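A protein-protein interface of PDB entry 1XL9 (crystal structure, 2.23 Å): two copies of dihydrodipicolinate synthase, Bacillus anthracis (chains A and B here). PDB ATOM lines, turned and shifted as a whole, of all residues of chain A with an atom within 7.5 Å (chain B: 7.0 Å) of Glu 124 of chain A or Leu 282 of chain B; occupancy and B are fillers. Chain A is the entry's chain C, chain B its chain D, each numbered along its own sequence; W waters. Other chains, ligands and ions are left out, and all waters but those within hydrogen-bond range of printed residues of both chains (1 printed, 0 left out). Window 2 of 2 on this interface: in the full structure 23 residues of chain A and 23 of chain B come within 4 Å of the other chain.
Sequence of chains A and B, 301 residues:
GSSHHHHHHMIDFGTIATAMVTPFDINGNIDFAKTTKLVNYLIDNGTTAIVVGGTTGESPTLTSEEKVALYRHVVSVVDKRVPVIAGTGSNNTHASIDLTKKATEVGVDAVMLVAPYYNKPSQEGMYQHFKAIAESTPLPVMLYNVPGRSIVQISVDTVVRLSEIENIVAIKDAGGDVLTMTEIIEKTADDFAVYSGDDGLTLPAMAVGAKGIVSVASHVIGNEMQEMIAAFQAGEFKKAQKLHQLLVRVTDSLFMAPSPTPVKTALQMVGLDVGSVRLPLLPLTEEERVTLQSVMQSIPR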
ATOM      1  N   PRO A 121      14.835 -10.849 -27.722  1.00  0.00           N
ATOM      2  CA  PRO A 121      13.800  -9.917 -27.254  1.00  0.00           C
ATOM      3  C   PRO A 121      12.997 -10.433 -26.048  1.00  0.00           C
ATOM      4  O   PRO A 121      12.925 -11.637 -25.800  1.00  0.00           O
ATOM      5  CB  PRO A 121      12.885  -9.778 -28.465  1.00  0.00           C
ATOM      6  CG  PRO A 121      13.081 -11.106 -29.238  1.00  0.00           C
ATOM      7  CD  PRO A 121      14.546 -11.406 -29.067  1.00  0.00           C
ATOM      8  N   SER A 122      12.413  -9.506 -25.296  1.00  0.00           N
ATOM      9  CA  SER A 122      11.451  -9.846 -24.247  1.00  0.00           C
ATOM     10  C   SER A 122      10.124 -10.229 -24.904  1.00  0.00           C
ATOM     11  O   SER A 122       9.967 -10.128 -26.116  1.00  0.00           O
ATOM     12  CB  SER A 122      11.205  -8.635 -23.360  1.00  0.00           C
ATOM     13  OG  SER A 122      10.609  -7.594 -24.118  1.00  0.00           O
ATOM     14  N   GLN A 123       9.175 -10.651 -24.081  1.00  0.00           N
ATOM     15  CA  GLN A 123       7.816 -11.014 -24.499  1.00  0.00           C
ATOM     16  C   GLN A 123       7.065  -9.787 -24.967  1.00  0.00           C
ATOM     17  O   GLN A 123       6.426  -9.827 -26.004  1.00  0.00           O
ATOM     18  CB  GLN A 123       7.051 -11.677 -23.329  1.00  0.00           C
ATOM     19  CG  GLN A 123       7.654 -13.006 -22.853  1.00  0.00           C
ATOM     20  CD  GLN A 123       7.641 -14.110 -23.923  1.00  0.00           C
ATOM     21  OE1 GLN A 123       6.686 -14.257 -24.693  1.00  0.00           O
ATOM     22  NE2 GLN A 123       8.680 -14.907 -23.938  1.00  0.00           N
ATOM     23  N   GLU A 124       7.147  -8.694 -24.212  1.00  0.00           N
ATOM     24  CA  GLU A 124       6.560  -7.435 -24.673  1.00  0.00           C
ATOM     25  C   GLU A 124       7.195  -6.950 -25.963  1.00  0.00           C
ATOM     26  O   GLU A 124       6.522  -6.424 -26.836  1.00  0.00           O
ATOM     27  CB  GLU A 124       6.639  -6.334 -23.608  1.00  0.00           C
ATOM     28  CG  GLU A 124       5.905  -5.036 -24.002  1.00  0.00           C
ATOM     29  CD  GLU A 124       4.432  -5.246 -24.319  1.00  0.00           C
ATOM     30  OE1 GLU A 124       3.782  -6.060 -23.631  1.00  0.00           O
ATOM     31  OE2 GLU A 124       3.922  -4.584 -25.253  1.00  0.00           O
ATOM     32  N   GLY A 125       8.500  -7.108 -26.072  1.00  0.00           N
ATOM     33  CA  GLY A 125       9.209  -6.711 -27.281  1.00  0.00           C
ATOM     34  C   GLY A 125       8.745  -7.476 -28.502  1.00  0.00           C
ATOM     35  O   GLY A 125       8.467  -6.868 -29.515  1.00  0.00           O
ATOM     36  N   MET A 126       8.691  -8.808 -28.403  1.00  0.00           N
ATOM     37  CA  MET A 126       8.110  -9.704 -29.436  1.00  0.00           C
ATOM     38  C   MET A 126       6.633  -9.405 -29.795  1.00  0.00           C
ATOM     39  O   MET A 126       6.257  -9.426 -30.980  1.00  0.00           O
ATOM     40  CB  MET A 126       8.232 -11.167 -28.991  1.00  0.00           C
ATOM     41  CG  MET A 126       9.545 -11.801 -29.437  1.00  0.00           C
ATOM     42  SD  MET A 126       9.753 -13.511 -28.965  1.00  0.00           S
ATOM     43  CE  MET A 126      10.059 -13.426 -27.198  1.00  0.00           C
ATOM     44  N   TYR A 127       5.819  -9.142 -28.769  1.00  0.00           N
ATOM     45  CA  TYR A 127       4.446  -8.675 -28.946  1.00  0.00           C
ATOM     46  C   TYR A 127       4.390  -7.447 -29.853  1.00  0.00           C
ATOM     47  O   TYR A 127       3.647  -7.447 -30.824  1.00  0.00           O
ATOM     48  CB  TYR A 127       3.744  -8.390 -27.593  1.00  0.00           C
ATOM     49  CG  TYR A 127       2.347  -7.854 -27.797  1.00  0.00           C
ATOM     50  CD1 TYR A 127       1.305  -8.695 -28.230  1.00  0.00           C
ATOM     51  CD2 TYR A 127       2.065  -6.506 -27.624  1.00  0.00           C
ATOM     52  CE1 TYR A 127       0.019  -8.200 -28.474  1.00  0.00           C
ATOM     53  CE2 TYR A 127       0.769  -6.004 -27.848  1.00  0.00           C
ATOM     54  CZ  TYR A 127      -0.229  -6.853 -28.279  1.00  0.00           C
ATOM     55  OH  TYR A 127      -1.465  -6.346 -28.508  1.00  0.00           O
ATOM     56  N   GLN A 128       5.192  -6.418 -29.583  1.00  0.00           N
ATOM     57  CA  GLN A 128       5.182  -5.225 -30.463  1.00  0.00           C
ATOM     58  C   GLN A 128       5.763  -5.500 -31.866  1.00  0.00           C
ATOM     59  O   GLN A 128       5.298  -4.923 -32.845  1.00  0.00           O
ATOM     60  CB  GLN A 128       5.914  -4.051 -29.830  1.00  0.00           C
ATOM     61  CG  GLN A 128       5.359  -3.532 -28.488  1.00  0.00           C
ATOM     62  CD  GLN A 128       3.974  -2.899 -28.592  1.00  0.00           C
ATOM     63  OE1 GLN A 128       3.239  -2.862 -27.615  1.00  0.00           O
ATOM     64  NE2 GLN A 128       3.610  -2.434 -29.765  1.00  0.00           N
ATOM     65  N   HIS A 129       6.778  -6.352 -31.948  1.00  0.00           N
ATOM     66  CA  HIS A 129       7.408  -6.747 -33.226  1.00  0.00           C
ATOM     67  C   HIS A 129       6.354  -7.263 -34.167  1.00  0.00           C
ATOM     68  O   HIS A 129       6.190  -6.783 -35.281  1.00  0.00           O
ATOM     69  CB  HIS A 129       8.431  -7.859 -32.931  1.00  0.00           C
ATOM     70  CG  HIS A 129       9.017  -8.534 -34.137  1.00  0.00           C
ATOM     71  ND1 HIS A 129      10.003  -7.961 -34.916  1.00  0.00           N
ATOM     72  CD2 HIS A 129       8.842  -9.790 -34.620  1.00  0.00           C
ATOM     73  CE1 HIS A 129      10.371  -8.824 -35.852  1.00  0.00           C
ATOM     74  NE2 HIS A 129       9.681  -9.939 -35.699  1.00  0.00           N
ATOM     75  N   PHE A 130       5.633  -8.256 -33.661  1.00  0.00           N
ATOM     76  CA  PHE A 130       4.623  -8.989 -34.404  1.00  0.00           C
ATOM     77  C   PHE A 130       3.379  -8.153 -34.614  1.00  0.00           C
ATOM     78  O   PHE A 130       2.774  -8.225 -35.665  1.00  0.00           O
ATOM     79  CB  PHE A 130       4.228 -10.262 -33.654  1.00  0.00           C
ATOM     80  CG  PHE A 130       5.250 -11.365 -33.693  1.00  0.00           C
ATOM     81  CD1 PHE A 130       5.812 -11.791 -34.900  1.00  0.00           C
ATOM     82  CD2 PHE A 130       5.607 -12.022 -32.530  1.00  0.00           C
ATOM     83  CE1 PHE A 130       6.704 -12.832 -34.934  1.00  0.00           C
ATOM     84  CE2 PHE A 130       6.523 -13.043 -32.551  1.00  0.00           C
ATOM     85  CZ  PHE A 130       7.064 -13.460 -33.789  1.00  0.00           C
ATOM     86  N   LYS A 131       2.959  -7.394 -33.609  1.00  0.00           N
ATOM     87  CA  LYS A 131       1.798  -6.493 -33.774  1.00  0.00           C
ATOM     88  C   LYS A 131       2.036  -5.466 -34.892  1.00  0.00           C
ATOM     89  O   LYS A 131       1.111  -5.073 -35.569  1.00  0.00           O
ATOM     90  CB  LYS A 131       1.527  -5.757 -32.462  1.00  0.00           C
ATOM     91  CG  LYS A 131       0.494  -4.628 -32.479  1.00  0.00           C
ATOM     92  CD  LYS A 131       0.410  -4.025 -31.056  1.00  0.00           C
ATOM     93  CE  LYS A 131      -0.948  -3.407 -30.771  1.00  0.00           C
ATOM     94  NZ  LYS A 131      -1.268  -2.337 -31.772  1.00  0.00           N
ATOM     95  N   THR A 158       1.750 -14.571 -24.451  1.00  0.00           N
ATOM     96  CA  THR A 158       2.078 -13.683 -25.575  1.00  0.00           C
ATOM     97  C   THR A 158       1.376 -14.145 -26.838  1.00  0.00           C
ATOM     98  O   THR A 158       0.879 -13.307 -27.590  1.00  0.00           O
ATOM     99  CB  THR A 158       3.606 -13.579 -25.818  1.00  0.00           C
ATOM    100  OG1 THR A 158       4.232 -12.945 -24.701  1.00  0.00           O
ATOM    101  CG2 THR A 158       3.932 -12.777 -27.075  1.00  0.00           C
ATOM    102  N   ARG A 161      -2.434 -13.301 -26.618  1.00  0.00           N
ATOM    103  CA  ARG A 161      -2.571 -11.884 -26.962  1.00  0.00           C
ATOM    104  C   ARG A 161      -2.529 -11.585 -28.457  1.00  0.00           C
ATOM    105  O   ARG A 161      -3.253 -10.722 -28.948  1.00  0.00           O
ATOM    106  CB  ARG A 161      -1.480 -11.076 -26.273  1.00  0.00           C
ATOM    107  CG  ARG A 161      -1.638 -10.972 -24.772  1.00  0.00           C
ATOM    108  CD  ARG A 161      -0.455 -10.260 -24.138  1.00  0.00           C
ATOM    109  NE  ARG A 161      -0.461  -8.820 -24.384  1.00  0.00           N
ATOM    110  CZ  ARG A 161       0.609  -8.017 -24.290  1.00  0.00           C
ATOM    111  NH1 ARG A 161       1.812  -8.500 -23.982  1.00  0.00           N
ATOM    112  NH2 ARG A 161       0.479  -6.713 -24.540  1.00  0.00           N
ATOM    113  N   ALA B 257      17.051  -6.556 -18.561  1.00  0.00           N
ATOM    114  CA  ALA B 257      16.275  -6.444 -19.760  1.00  0.00           C
ATOM    115  C   ALA B 257      17.208  -6.733 -20.955  1.00  0.00           C
ATOM    116  O   ALA B 257      18.414  -6.771 -20.791  1.00  0.00           O
ATOM    117  CB  ALA B 257      15.704  -5.072 -19.830  1.00  0.00           C
ATOM    118  N   PRO B 258      16.665  -6.968 -22.154  1.00  0.00           N
ATOM    119  CA  PRO B 258      17.565  -7.279 -23.278  1.00  0.00           C
ATOM    120  C   PRO B 258      18.570  -6.162 -23.580  1.00  0.00           C
ATOM    121  O   PRO B 258      18.198  -5.007 -23.689  1.00  0.00           O
ATOM    122  CB  PRO B 258      16.599  -7.491 -24.448  1.00  0.00           C
ATOM    123  CG  PRO B 258      15.313  -7.897 -23.782  1.00  0.00           C
ATOM    124  CD  PRO B 258      15.255  -7.019 -22.562  1.00  0.00           C
ATOM    125  N   THR B 261      19.702  -2.179 -24.121  1.00  0.00           N
ATOM    126  CA  THR B 261      18.859  -1.134 -23.559  1.00  0.00           C
ATOM    127  C   THR B 261      19.220  -0.659 -22.136  1.00  0.00           C
ATOM    128  O   THR B 261      19.229   0.546 -21.870  1.00  0.00           O
ATOM    129  CB  THR B 261      17.360  -1.538 -23.600  1.00  0.00           C
ATOM    130  OG1 THR B 261      17.041  -2.028 -24.902  1.00  0.00           O
ATOM    131  CG2 THR B 261      16.430  -0.339 -23.269  1.00  0.00           C
ATOM    132  N   PRO B 262      19.439  -1.582 -21.199  1.00  0.00           N
ATOM    133  CA  PRO B 262      19.849  -1.103 -19.882  1.00  0.00           C
ATOM    134  C   PRO B 262      21.039  -0.159 -19.903  1.00  0.00           C
ATOM    135  O   PRO B 262      20.991   0.869 -19.246  1.00  0.00           O
ATOM    136  CB  PRO B 262      20.168  -2.401 -19.122  1.00  0.00           C
ATOM    137  CG  PRO B 262      19.265  -3.424 -19.770  1.00  0.00           C
ATOM    138  CD  PRO B 262      19.245  -3.044 -21.221  1.00  0.00           C
ATOM    139  N   SER B 276      17.522   5.723 -27.584  1.00  0.00           N
ATOM    140  CA  SER B 276      16.913   4.458 -27.309  1.00  0.00           C
ATOM    141  C   SER B 276      17.341   3.451 -28.380  1.00  0.00           C
ATOM    142  O   SER B 276      18.368   3.607 -29.032  1.00  0.00           O
ATOM    143  CB  SER B 276      15.389   4.623 -27.242  1.00  0.00           C
ATOM    144  OG  SER B 276      14.810   3.564 -26.504  1.00  0.00           O
ATOM    145  N   VAL B 277      16.494   2.451 -28.584  1.00  0.00           N
ATOM    146  CA  VAL B 277      16.822   1.219 -29.293  1.00  0.00           C
ATOM    147  C   VAL B 277      15.784   0.962 -30.376  1.00  0.00           C
ATOM    148  O   VAL B 277      14.661   1.456 -30.309  1.00  0.00           O
ATOM    149  CB  VAL B 277      16.843   0.009 -28.290  1.00  0.00           C
ATOM    150  CG1 VAL B 277      18.082   0.057 -27.423  1.00  0.00           C
ATOM    151  CG2 VAL B 277      15.564  -0.016 -27.403  1.00  0.00           C
ATOM    152  N   ARG B 278      16.164   0.175 -31.372  1.00  0.00           N
ATOM    153  CA  ARG B 278      15.282  -0.164 -32.480  1.00  0.00           C
ATOM    154  C   ARG B 278      14.491  -1.443 -32.179  1.00  0.00           C
ATOM    155  O   ARG B 278      14.960  -2.308 -31.435  1.00  0.00           O
ATOM    156  CB  ARG B 278      16.118  -0.344 -33.782  1.00  0.00           C
ATOM    157  CG  ARG B 278      16.607   0.993 -34.384  1.00  0.00           C
ATOM    158  CD  ARG B 278      17.359   0.829 -35.721  1.00  0.00           C
ATOM    159  NE  ARG B 278      17.962   2.092 -36.145  1.00  0.00           N
ATOM    160  CZ  ARG B 278      18.787   2.225 -37.179  1.00  0.00           C
ATOM    161  NH1 ARG B 278      19.088   1.182 -37.931  1.00  0.00           N
ATOM    162  NH2 ARG B 278      19.291   3.413 -37.482  1.00  0.00           N
ATOM    163  N   LEU B 279      13.310  -1.572 -32.793  1.00  0.00           N
ATOM    164  CA  LEU B 279      12.515  -2.806 -32.716  1.00  0.00           C
ATOM    165  C   LEU B 279      13.227  -3.967 -33.379  1.00  0.00           C
ATOM    166  O   LEU B 279      13.860  -3.780 -34.425  1.00  0.00           O
ATOM    167  CB  LEU B 279      11.128  -2.603 -33.312  1.00  0.00           C
ATOM    168  CG  LEU B 279      10.204  -1.749 -32.410  1.00  0.00           C
ATOM    169  CD1 LEU B 279       9.079  -1.153 -33.223  1.00  0.00           C
ATOM    170  CD2 LEU B 279       9.651  -2.562 -31.219  1.00  0.00           C
ATOM    171  N   PRO B 280      13.133  -5.177 -32.770  1.00  0.00           N
ATOM    172  CA  PRO B 280      12.208  -5.620 -31.704  1.00  0.00           C
ATOM    173  C   PRO B 280      12.552  -5.281 -30.239  1.00  0.00           C
ATOM    174  O   PRO B 280      11.945  -5.854 -29.343  1.00  0.00           O
ATOM    175  CB  PRO B 280      12.204  -7.142 -31.887  1.00  0.00           C
ATOM    176  CG  PRO B 280      13.515  -7.459 -32.381  1.00  0.00           C
ATOM    177  CD  PRO B 280      14.060  -6.264 -33.128  1.00  0.00           C
ATOM    178  N   LEU B 281      13.499  -4.378 -29.990  1.00  0.00           N
ATOM    179  CA  LEU B 281      13.843  -3.968 -28.632  1.00  0.00           C
ATOM    180  C   LEU B 281      13.080  -2.717 -28.176  1.00  0.00           C
ATOM    181  O   LEU B 281      12.584  -1.961 -28.994  1.00  0.00           O
ATOM    182  CB  LEU B 281      15.350  -3.721 -28.522  1.00  0.00           C
ATOM    183  CG  LEU B 281      16.367  -4.794 -28.962  1.00  0.00           C
ATOM    184  CD1 LEU B 281      17.748  -4.243 -28.789  1.00  0.00           C
ATOM    185  CD2 LEU B 281      16.253  -6.084 -28.154  1.00  0.00           C
ATOM    186  N   LEU B 282      13.022  -2.501 -26.861  1.00  0.00           N
ATOM    187  CA  LEU B 282      12.125  -1.506 -26.271  1.00  0.00           C
ATOM    188  C   LEU B 282      12.728  -0.762 -25.094  1.00  0.00           C
ATOM    189  O   LEU B 282      13.518  -1.324 -24.354  1.00  0.00           O
ATOM    190  CB  LEU B 282      10.839  -2.174 -25.785  1.00  0.00           C
ATOM    191  CG  LEU B 282       9.796  -2.653 -26.799  1.00  0.00           C
ATOM    192  CD1 LEU B 282       8.694  -3.314 -26.043  1.00  0.00           C
ATOM    193  CD2 LEU B 282       9.234  -1.497 -27.602  1.00  0.00           C
ATOM    194  N   PRO B 283      12.342   0.515 -24.919  1.00  0.00           N
ATOM    195  CA  PRO B 283      12.733   1.283 -23.737  1.00  0.00           C
ATOM    196  C   PRO B 283      12.442   0.566 -22.440  1.00  0.00           C
ATOM    197  O   PRO B 283      11.500  -0.215 -22.360  1.00  0.00           O
ATOM    198  CB  PRO B 283      11.871   2.557 -23.829  1.00  0.00           C
ATOM    199  CG  PRO B 283      11.619   2.738 -25.292  1.00  0.00           C
ATOM    200  CD  PRO B 283      11.532   1.323 -25.861  1.00  0.00           C
ATOM    201  N   LEU B 284      13.278   0.803 -21.437  1.00  0.00           N
ATOM    202  CA  LEU B 284      12.958   0.336 -20.073  1.00  0.00           C
ATOM    203  C   LEU B 284      11.562   0.863 -19.668  1.00  0.00           C
ATOM    204  O   LEU B 284      11.095   1.873 -20.193  1.00  0.00           O
ATOM    205  CB  LEU B 284      14.048   0.735 -19.050  1.00  0.00           C
ATOM    206  CG  LEU B 284      15.127  -0.324 -18.787  1.00  0.00           C
ATOM    207  CD1 LEU B 284      15.765  -0.758 -20.083  1.00  0.00           C
ATOM    208  CD2 LEU B 284      16.216   0.161 -17.806  1.00  0.00           C
ATOM    209  N   THR B 285      10.877   0.117 -18.813  1.00  0.00           N
ATOM    210  CA  THR B 285       9.656   0.605 -18.164  1.00  0.00           C
ATOM    211  C   THR B 285      10.088   1.523 -17.050  1.00  0.00           C
ATOM    212  O   THR B 285      11.272   1.585 -16.732  1.00  0.00           O
ATOM    213  CB  THR B 285       8.832  -0.521 -17.541  1.00  0.00           C
ATOM    214  OG1 THR B 285       9.623  -1.202 -16.566  1.00  0.00           O
ATOM    215  CG2 THR B 285       8.369  -1.511 -18.587  1.00  0.00           C
ATOM    216  N   GLU B 288      11.470  -0.687 -14.337  1.00  0.00           N
ATOM    217  CA  GLU B 288      12.818  -1.122 -14.766  1.00  0.00           C
ATOM    218  C   GLU B 288      13.899  -0.040 -14.637  1.00  0.00           C
ATOM    219  O   GLU B 288      15.053  -0.330 -14.294  1.00  0.00           O
ATOM    220  CB  GLU B 288      12.791  -1.614 -16.220  1.00  0.00           C
ATOM    221  CG  GLU B 288      12.211  -3.023 -16.425  1.00  0.00           C
ATOM    222  CD  GLU B 288      12.151  -3.433 -17.894  1.00  0.00           C
ATOM    223  OE1 GLU B 288      11.889  -2.570 -18.757  1.00  0.00           O
ATOM    224  OE2 GLU B 288      12.363  -4.631 -18.197  1.00  0.00           O
HETATM  225  O   HOH W   1      12.568  -7.068 -26.932  1.00  0.00           O
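Among the printed residues, merely in contact across the chains: Gly 125 of chain A with Pro 280 of chain B, Ser 122 of chain A with Pro 258 of chain B, Gly 125 of chain A with Leu 282 of chain B, His 129 of chain A with Pro 280 of chain B and Glu 124 of chain A with Leu 282 of chain B.
OG of Ser 122 of chain A is in hydrogen-bond range of N of Gly 125 of chain A, 2.9 Å away. The side-chain carboxylate of Glu 124 of chain A lies close to the side-chain amide oxygen of Gln 128 of chain A (3.0 Å). The side-chain carboxylate (OE1) of Glu 124 of chain A is in salt-bridge range of the guanidinium group (NH1) of Arg 161 of chain A (3.2 Å). O of Pro 258 of chain B lies within hydrogen-bond range of OG1 of Thr 261 of chain B (3.4 Å).
Hydrophobic or aromatic side chains of chain A that line the printed part of chain B: His 129. Of the 15 printed residues of chain B, 3 touch a printed residue of chain A. Printed residues of chain B that touch a printed residue of chain A: Pro 258, Pro 280 and Leu 282. Hydrophobic or aromatic side chains of chain B that line the printed part of chain A: Pro 258, Pro 280 and Leu 282.
Water W1 lies within hydrogen-bond range of O of Pro 280 of chain B (2.8 Å) and N of Ser 122 of chain A (2.9 Å).
No position is printed for both chains.
Of the printed residues of chain B, Ser 122 of chain A touches Pro 258 (3.6 Å). Printed residues of chain B within 4 Å of Glu 124 of chain A: Leu 282 (3.9 Å). Printed residues of chain B within 4 Å of Gly 125 of chain A: Pro 280 and Leu 282. Of the printed residues of chain A, Pro 258 of chain B touches Ser 122. Printed residues of chain A within 4 Å of Leu 282 of chain B: Glu 124 and Gly 125. Leu 284 of chain B touches none of the printed residues of chain A. The nearest printed residue of chain B that does not touch His 129 of chain A is Leu 279 of chain B (4.8 Å).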
